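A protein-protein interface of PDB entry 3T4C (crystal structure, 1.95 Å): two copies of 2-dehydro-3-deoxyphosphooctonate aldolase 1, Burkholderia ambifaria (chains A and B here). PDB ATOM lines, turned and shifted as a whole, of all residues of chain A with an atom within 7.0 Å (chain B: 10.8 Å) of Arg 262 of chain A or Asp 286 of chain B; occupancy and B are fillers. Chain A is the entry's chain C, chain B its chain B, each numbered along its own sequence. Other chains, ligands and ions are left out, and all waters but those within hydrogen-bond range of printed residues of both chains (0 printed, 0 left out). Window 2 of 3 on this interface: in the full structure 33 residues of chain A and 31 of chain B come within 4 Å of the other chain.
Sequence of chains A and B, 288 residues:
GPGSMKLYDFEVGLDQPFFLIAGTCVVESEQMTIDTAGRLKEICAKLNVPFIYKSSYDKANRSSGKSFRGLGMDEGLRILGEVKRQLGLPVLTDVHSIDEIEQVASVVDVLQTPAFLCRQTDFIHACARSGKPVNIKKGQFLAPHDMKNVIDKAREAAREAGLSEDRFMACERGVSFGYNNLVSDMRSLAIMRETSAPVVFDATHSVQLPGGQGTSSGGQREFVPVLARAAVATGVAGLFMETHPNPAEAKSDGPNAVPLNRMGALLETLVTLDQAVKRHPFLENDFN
No position is printed for both chains.
Of the 5 pairs that touch across the chains among the printed residues, none has its exchanged pair printed and touching as well.
The side-chain carboxylate of Asp 286 of chain B lies within salt-bridge range of the guanidinium group of Arg 262 of chain A, at 2.4 Å.
Hydrophobic or aromatic side chains of chain B that line the printed part of chain A: Leu 283 and Phe 287.
Of the 14 printed residues of chain A, 4 touch a printed residue of chain B.
Among the printed residues, 5 pairs touch across the chains.
Of the printed residues of chain B, Arg 221 of chain A touches Phe 287 (3.8 Å).
Pro 259 of chain A touches one residue of chain B.
No residue of chain B comes within 4 Å of Asn 261 of chain A.
Arg 262 of chain A touches just these residues of chain B: Leu 283 (3.3 Å) and Asp 286 (2.4 Å).
No residue of chain B comes within 4 Å of Met 263 of chain A.
No residue of chain B comes within 4 Å of Gly 264 of chain A.
No residue of chain B comes within 4 Å of Ala 265 of chain A.
Of chain B, only Leu 283 comes within 4 Å of Leu 266 of chain A.
Val 277 of chain B touches none of the printed residues of chain A.
Of the printed residues of chain A, Leu 283 of chain B touches Arg 262 (3.3 Å) and Leu 266 (3.9 Å).
Of chain A, only Arg 262 comes within 4 Å of Asp 286 of chain B.
Printed residues of chain A within 4 Å of Phe 287 of chain B: Arg 221 (3.8 Å) and Pro 259 (3.6 Å).
The nearest residue of chain B that does not touch Arg 262 of chain A is Phe 287 of chain B (4.7 Å).
The nearest residue of chain A that does not touch Asp 286 of chain B is Arg 221 of chain A (4.6 Å).
The nearest printed residue of chain A that does not touch Phe 287 of chain B is Val 258 of chain A (4.5 Å).
NE of Arg 221 of chain A touches CB of Phe 287 of chain B (3.8 Å).
Phe 287 of chain B touches Pro 259 of chain A (CZ to CD, 3.6 Å).
Arg 262 of chain A touches Leu 283 of chain B.
Leu 283 of chain B touches Leu 266 of chain A (CD2 to CB, 3.9 Å).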
ATOM      1  N   ILE A  43       7.492  12.702 -18.561  1.00  0.00           N
ATOM      2  CA  ILE A  43       7.944  13.341 -17.323  1.00  0.00           C
ATOM      3  C   ILE A  43       8.586  14.719 -17.588  1.00  0.00           C
ATOM      4  O   ILE A  43       8.300  15.718 -16.885  1.00  0.00           O
ATOM      5  CB  ILE A  43       8.965  12.441 -16.567  1.00  0.00           C
ATOM      6  CG1 ILE A  43       8.236  11.264 -15.901  1.00  0.00           C
ATOM      7  CG2 ILE A  43       9.750  13.255 -15.535  1.00  0.00           C
ATOM      8  CD1 ILE A  43       9.099  10.041 -15.675  1.00  0.00           C
ATOM      9  N   ARG A 221      23.529   4.940  -5.148  1.00  0.00           N
ATOM     10  CA  ARG A 221      22.478   5.700  -5.745  1.00  0.00           C
ATOM     11  C   ARG A 221      22.013   6.804  -4.816  1.00  0.00           C
ATOM     12  O   ARG A 221      21.560   7.802  -5.292  1.00  0.00           O
ATOM     13  CB  ARG A 221      21.284   4.809  -6.164  1.00  0.00           C
ATOM     14  CG  ARG A 221      20.527   4.250  -4.984  1.00  0.00           C
ATOM     15  CD  ARG A 221      19.356   3.356  -5.450  1.00  0.00           C
ATOM     16  NE  ARG A 221      18.590   2.913  -4.291  1.00  0.00           N
ATOM     17  CZ  ARG A 221      17.358   2.401  -4.343  1.00  0.00           C
ATOM     18  NH1 ARG A 221      16.727   2.262  -5.502  1.00  0.00           N
ATOM     19  NH2 ARG A 221      16.750   2.027  -3.220  1.00  0.00           N
ATOM     20  N   THR A 243      18.495   6.144 -15.048  1.00  0.00           N
ATOM     21  CA  THR A 243      17.266   5.839 -14.338  1.00  0.00           C
ATOM     22  C   THR A 243      17.009   4.331 -14.325  1.00  0.00           C
ATOM     23  O   THR A 243      17.417   3.627 -15.235  1.00  0.00           O
ATOM     24  CB  THR A 243      16.048   6.564 -14.951  1.00  0.00           C
ATOM     25  OG1 THR A 243      14.933   6.345 -14.099  1.00  0.00           O
ATOM     26  CG2 THR A 243      15.718   6.005 -16.316  1.00  0.00           C
ATOM     27  N   PRO A 247      11.213  -0.200 -10.772  1.00  0.00           N
ATOM     28  CA  PRO A 247      11.330   0.152  -9.339  1.00  0.00           C
ATOM     29  C   PRO A 247      11.140  -1.053  -8.417  1.00  0.00           C
ATOM     30  O   PRO A 247      11.731  -1.098  -7.347  1.00  0.00           O
ATOM     31  CB  PRO A 247      10.197   1.171  -9.123  1.00  0.00           C
ATOM     32  CG  PRO A 247       9.238   0.900 -10.236  1.00  0.00           C
ATOM     33  CD  PRO A 247      10.140   0.584 -11.415  1.00  0.00           C
ATOM     34  N   VAL A 258      18.426   6.430 -10.492  1.00  0.00           N
ATOM     35  CA  VAL A 258      17.249   6.949  -9.779  1.00  0.00           C
ATOM     36  C   VAL A 258      16.068   6.137 -10.317  1.00  0.00           C
ATOM     37  O   VAL A 258      15.923   5.993 -11.525  1.00  0.00           O
ATOM     38  CB  VAL A 258      17.070   8.464 -10.054  1.00  0.00           C
ATOM     39  CG1 VAL A 258      15.757   9.021  -9.510  1.00  0.00           C
ATOM     40  CG2 VAL A 258      18.270   9.232  -9.464  1.00  0.00           C
ATOM     41  N   PRO A 259      15.255   5.574  -9.427  1.00  0.00           N
ATOM     42  CA  PRO A 259      14.105   4.874  -9.925  1.00  0.00           C
ATOM     43  C   PRO A 259      13.233   5.795 -10.773  1.00  0.00           C
ATOM     44  O   PRO A 259      13.042   6.958 -10.420  1.00  0.00           O
ATOM     45  CB  PRO A 259      13.372   4.388  -8.659  1.00  0.00           C
ATOM     46  CG  PRO A 259      14.358   4.489  -7.559  1.00  0.00           C
ATOM     47  CD  PRO A 259      15.301   5.615  -7.957  1.00  0.00           C
ATOM     48  N   LEU A 260      12.751   5.266 -11.903  1.00  0.00           N
ATOM     49  CA  LEU A 260      11.969   6.033 -12.875  1.00  0.00           C
ATOM     50  C   LEU A 260      10.769   6.728 -12.242  1.00  0.00           C
ATOM     51  O   LEU A 260      10.472   7.874 -12.579  1.00  0.00           O
ATOM     52  CB  LEU A 260      11.502   5.138 -14.013  1.00  0.00           C
ATOM     53  CG  LEU A 260      10.774   5.785 -15.212  1.00  0.00           C
ATOM     54  CD1 LEU A 260      11.648   6.913 -15.775  1.00  0.00           C
ATOM     55  CD2 LEU A 260      10.439   4.753 -16.292  1.00  0.00           C
ATOM     56  N   ASN A 261      10.103   6.051 -11.307  1.00  0.00           N
ATOM     57  CA  ASN A 261       8.901   6.623 -10.657  1.00  0.00           C
ATOM     58  C   ASN A 261       9.183   7.737  -9.626  1.00  0.00           C
ATOM     59  O   ASN A 261       8.274   8.311  -9.068  1.00  0.00           O
ATOM     60  CB  ASN A 261       8.016   5.505 -10.063  1.00  0.00           C
ATOM     61  CG  ASN A 261       8.676   4.766  -8.900  1.00  0.00           C
ATOM     62  OD1 ASN A 261       9.842   5.000  -8.550  1.00  0.00           O
ATOM     63  ND2 ASN A 261       7.930   3.796  -8.337  1.00  0.00           N
ATOM     64  N   ARG A 262      10.462   8.012  -9.356  1.00  0.00           N
ATOM     65  CA  ARG A 262      10.899   9.160  -8.555  1.00  0.00           C
ATOM     66  C   ARG A 262      11.574  10.278  -9.384  1.00  0.00           C
ATOM     67  O   ARG A 262      11.962  11.316  -8.837  1.00  0.00           O
ATOM     68  CB  ARG A 262      11.879   8.674  -7.465  1.00  0.00           C
ATOM     69  CG  ARG A 262      11.275   7.599  -6.559  1.00  0.00           C
ATOM     70  CD  ARG A 262      10.006   8.047  -5.811  1.00  0.00           C
ATOM     71  NE  ARG A 262      10.398   8.504  -4.476  1.00  0.00           N
ATOM     72  CZ  ARG A 262      10.131   9.694  -3.928  1.00  0.00           C
ATOM     73  NH1 ARG A 262       9.372  10.626  -4.531  1.00  0.00           N
ATOM     74  NH2 ARG A 262      10.603   9.925  -2.729  1.00  0.00           N
ATOM     75  N   MET A 263      11.778  10.043 -10.683  1.00  0.00           N
ATOM     76  CA  MET A 263      12.424  11.038 -11.517  1.00  0.00           C
ATOM     77  C   MET A 263      11.663  12.360 -11.581  1.00  0.00           C
ATOM     78  O   MET A 263      12.306  13.414 -11.533  1.00  0.00           O
ATOM     79  CB  MET A 263      12.668  10.525 -12.963  1.00  0.00           C
ATOM     80  CG  MET A 263      13.781   9.524 -13.061  1.00  0.00           C
ATOM     81  SD  MET A 263      15.452  10.219 -12.887  1.00  0.00           S
ATOM     82  CE  MET A 263      15.709  11.226 -14.328  1.00  0.00           C
ATOM     83  N   GLY A 264      10.332  12.296 -11.734  1.00  0.00           N
ATOM     84  CA  GLY A 264       9.486  13.494 -11.747  1.00  0.00           C
ATOM     85  C   GLY A 264       9.712  14.426 -10.538  1.00  0.00           C
ATOM     86  O   GLY A 264      10.003  15.633 -10.670  1.00  0.00           O
ATOM     87  N   ALA A 265       9.649  13.833  -9.359  1.00  0.00           N
ATOM     88  CA  ALA A 265       9.827  14.559  -8.123  1.00  0.00           C
ATOM     89  C   ALA A 265      11.207  15.218  -8.039  1.00  0.00           C
ATOM     90  O   ALA A 265      11.312  16.383  -7.652  1.00  0.00           O
ATOM     91  CB  ALA A 265       9.601  13.618  -6.941  1.00  0.00           C
ATOM     92  N   LEU A 266      12.251  14.501  -8.440  1.00  0.00           N
ATOM     93  CA  LEU A 266      13.605  15.055  -8.412  1.00  0.00           C
ATOM     94  C   LEU A 266      13.734  16.181  -9.407  1.00  0.00           C
ATOM     95  O   LEU A 266      14.253  17.201  -9.055  1.00  0.00           O
ATOM     96  CB  LEU A 266      14.675  13.987  -8.679  1.00  0.00           C
ATOM     97  CG  LEU A 266      16.128  14.436  -8.714  1.00  0.00           C
ATOM     98  CD1 LEU A 266      16.497  15.070  -7.377  1.00  0.00           C
ATOM     99  CD2 LEU A 266      16.998  13.240  -9.061  1.00  0.00           C
ATOM    100  N   LEU A 267      13.254  15.985 -10.642  1.00  0.00           N
ATOM    101  CA  LEU A 267      13.301  17.036 -11.649  1.00  0.00           C
ATOM    102  C   LEU A 267      12.569  18.309 -11.246  1.00  0.00           C
ATOM    103  O   LEU A 267      13.058  19.394 -11.527  1.00  0.00           O
ATOM    104  CB  LEU A 267      12.806  16.527 -13.012  1.00  0.00           C
ATOM    105  CG  LEU A 267      13.823  15.549 -13.621  1.00  0.00           C
ATOM    106  CD1 LEU A 267      13.135  14.830 -14.768  1.00  0.00           C
ATOM    107  CD2 LEU A 267      15.126  16.224 -14.099  1.00  0.00           C
ATOM    108  N   ALA B 190      25.504  14.860   3.600  1.00  0.00           N
ATOM    109  CA  ALA B 190      24.426  13.889   3.765  1.00  0.00           C
ATOM    110  C   ALA B 190      24.819  12.795   4.731  1.00  0.00           C
ATOM    111  O   ALA B 190      24.035  12.446   5.600  1.00  0.00           O
ATOM    112  CB  ALA B 190      23.990  13.288   2.436  1.00  0.00           C
ATOM    113  N   ARG B 193      24.523  13.473   8.520  1.00  0.00           N
ATOM    114  CA  ARG B 193      23.184  13.397   9.090  1.00  0.00           C
ATOM    115  C   ARG B 193      23.056  12.239  10.062  1.00  0.00           C
ATOM    116  O   ARG B 193      22.254  12.309  10.990  1.00  0.00           O
ATOM    117  CB  ARG B 193      22.100  13.304   8.022  1.00  0.00           C
ATOM    118  CG  ARG B 193      22.044  14.540   7.142  1.00  0.00           C
ATOM    119  CD  ARG B 193      21.144  14.370   5.943  1.00  0.00           C
ATOM    120  NE  ARG B 193      21.348  15.498   5.048  1.00  0.00           N
ATOM    121  CZ  ARG B 193      20.987  15.540   3.770  1.00  0.00           C
ATOM    122  NH1 ARG B 193      20.410  14.510   3.193  1.00  0.00           N
ATOM    123  NH2 ARG B 193      21.245  16.603   3.044  1.00  0.00           N
ATOM    124  N   VAL B 277      14.678  22.908  -1.245  1.00  0.00           N
ATOM    125  CA  VAL B 277      15.083  21.514  -0.972  1.00  0.00           C
ATOM    126  C   VAL B 277      14.438  20.959   0.271  1.00  0.00           C
ATOM    127  O   VAL B 277      14.478  19.744   0.523  1.00  0.00           O
ATOM    128  CB  VAL B 277      16.626  21.377  -0.979  1.00  0.00           C
ATOM    129  CG1 VAL B 277      17.162  21.971  -2.299  1.00  0.00           C
ATOM    130  CG2 VAL B 277      17.327  22.032   0.211  1.00  0.00           C
ATOM    131  N   HIS B 280      10.063  19.273   0.486  1.00  0.00           N
ATOM    132  CA  HIS B 280       9.736  17.870   0.550  1.00  0.00           C
ATOM    133  C   HIS B 280      10.880  17.153   1.211  1.00  0.00           C
ATOM    134  O   HIS B 280      11.968  17.701   1.306  1.00  0.00           O
ATOM    135  CB  HIS B 280       9.558  17.314  -0.867  1.00  0.00           C
ATOM    136  CG  HIS B 280       8.447  17.970  -1.632  1.00  0.00           C
ATOM    137  ND1 HIS B 280       7.147  17.793  -1.313  1.00  0.00           N
ATOM    138  CD2 HIS B 280       8.479  18.863  -2.708  1.00  0.00           C
ATOM    139  CE1 HIS B 280       6.381  18.513  -2.157  1.00  0.00           C
ATOM    140  NE2 HIS B 280       7.201  19.179  -3.002  1.00  0.00           N
ATOM    141  N   PRO B 281      10.659  15.918   1.675  1.00  0.00           N
ATOM    142  CA  PRO B 281      11.785  15.128   2.178  1.00  0.00           C
ATOM    143  C   PRO B 281      12.891  14.976   1.127  1.00  0.00           C
ATOM    144  O   PRO B 281      12.630  15.002  -0.052  1.00  0.00           O
ATOM    145  CB  PRO B 281      11.141  13.776   2.501  1.00  0.00           C
ATOM    146  CG  PRO B 281       9.718  14.106   2.759  1.00  0.00           C
ATOM    147  CD  PRO B 281       9.412  15.130   1.696  1.00  0.00           C
ATOM    148  N   PHE B 282      14.138  14.887   1.553  1.00  0.00           N
ATOM    149  CA  PHE B 282      15.242  14.703   0.601  1.00  0.00           C
ATOM    150  C   PHE B 282      15.098  13.350  -0.023  1.00  0.00           C
ATOM    151  O   PHE B 282      14.880  12.374   0.700  1.00  0.00           O
ATOM    152  CB  PHE B 282      16.590  14.779   1.333  1.00  0.00           C
ATOM    153  CG  PHE B 282      16.924  16.140   1.831  1.00  0.00           C
ATOM    154  CD1 PHE B 282      17.285  17.133   0.952  1.00  0.00           C
ATOM    155  CD2 PHE B 282      16.797  16.459   3.170  1.00  0.00           C
ATOM    156  CE1 PHE B 282      17.612  18.394   1.383  1.00  0.00           C
ATOM    157  CE2 PHE B 282      17.041  17.740   3.602  1.00  0.00           C
ATOM    158  CZ  PHE B 282      17.467  18.717   2.713  1.00  0.00           C
ATOM    159  N   LEU B 283      15.266  13.272  -1.347  1.00  0.00           N
ATOM    160  CA  LEU B 283      14.998  12.033  -2.063  1.00  0.00           C
ATOM    161  C   LEU B 283      15.848  10.886  -1.538  1.00  0.00           C
ATOM    162  O   LEU B 283      15.378   9.716  -1.456  1.00  0.00           O
ATOM    163  CB  LEU B 283      15.271  12.198  -3.567  1.00  0.00           C
ATOM    164  CG  LEU B 283      14.785  11.054  -4.453  1.00  0.00           C
ATOM    165  CD1 LEU B 283      13.282  11.016  -4.267  1.00  0.00           C
ATOM    166  CD2 LEU B 283      15.129  11.183  -5.943  1.00  0.00           C
ATOM    167  N   GLU B 284      17.089  11.202  -1.209  1.00  0.00           N
ATOM    168  CA  GLU B 284      18.047  10.174  -0.789  1.00  0.00           C
ATOM    169  C   GLU B 284      17.579   9.403   0.477  1.00  0.00           C
ATOM    170  O   GLU B 284      18.028   8.288   0.676  1.00  0.00           O
ATOM    171  CB  GLU B 284      19.459  10.740  -0.593  1.00  0.00           C
ATOM    172  CG  GLU B 284      19.594  11.881   0.443  1.00  0.00           C
ATOM    173  CD  GLU B 284      19.431  13.291  -0.170  1.00  0.00           C
ATOM    174  OE1 GLU B 284      18.877  13.410  -1.308  1.00  0.00           O
ATOM    175  OE2 GLU B 284      19.864  14.289   0.478  1.00  0.00           O
ATOM    176  N   ASN B 285      16.671   9.988   1.276  1.00  0.00           N
ATOM    177  CA  ASN B 285      16.043   9.325   2.443  1.00  0.00           C
ATOM    178  C   ASN B 285      15.238   8.108   2.072  1.00  0.00           C
ATOM    179  O   ASN B 285      15.136   7.164   2.840  1.00  0.00           O
ATOM    180  CB  ASN B 285      15.055  10.260   3.124  1.00  0.00           C
ATOM    181  CG  ASN B 285      15.734  11.386   3.869  1.00  0.00           C
ATOM    182  OD1 ASN B 285      16.955  11.572   3.766  1.00  0.00           O
ATOM    183  ND2 ASN B 285      14.942  12.144   4.642  1.00  0.00           N
ATOM    184  N   ASP B 286      14.647   8.165   0.882  1.00  0.00           N
ATOM    185  CA  ASP B 286      13.849   7.081   0.336  1.00  0.00           C
ATOM    186  C   ASP B 286      14.683   6.014  -0.376  1.00  0.00           C
ATOM    187  O   ASP B 286      14.130   5.067  -0.931  1.00  0.00           O
ATOM    188  CB  ASP B 286      12.788   7.695  -0.561  1.00  0.00           C
ATOM    189  CG  ASP B 286      12.008   8.762   0.166  1.00  0.00           C
ATOM    190  OD1 ASP B 286      12.025   8.723   1.419  1.00  0.00           O
ATOM    191  OD2 ASP B 286      11.401   9.638  -0.481  1.00  0.00           O
ATOM    192  N   PHE B 287      16.012   6.132  -0.313  1.00  0.00           N
ATOM    193  CA  PHE B 287      16.909   5.125  -0.884  1.00  0.00           C
ATOM    194  C   PHE B 287      17.615   4.329   0.231  1.00  0.00           C
ATOM    195  O   PHE B 287      18.809   4.498   0.501  1.00  0.00           O
ATOM    196  CB  PHE B 287      17.920   5.784  -1.846  1.00  0.00           C
ATOM    197  CG  PHE B 287      17.290   6.483  -3.045  1.00  0.00           C
ATOM    198  CD1 PHE B 287      18.036   7.356  -3.808  1.00  0.00           C
ATOM    199  CD2 PHE B 287      15.960   6.284  -3.400  1.00  0.00           C
ATOM    200  CE1 PHE B 287      17.496   7.979  -4.913  1.00  0.00           C
ATOM    201  CE2 PHE B 287      15.400   6.920  -4.492  1.00  0.00           C
ATOM    202  CZ  PHE B 287      16.169   7.773  -5.248  1.00  0.00           C
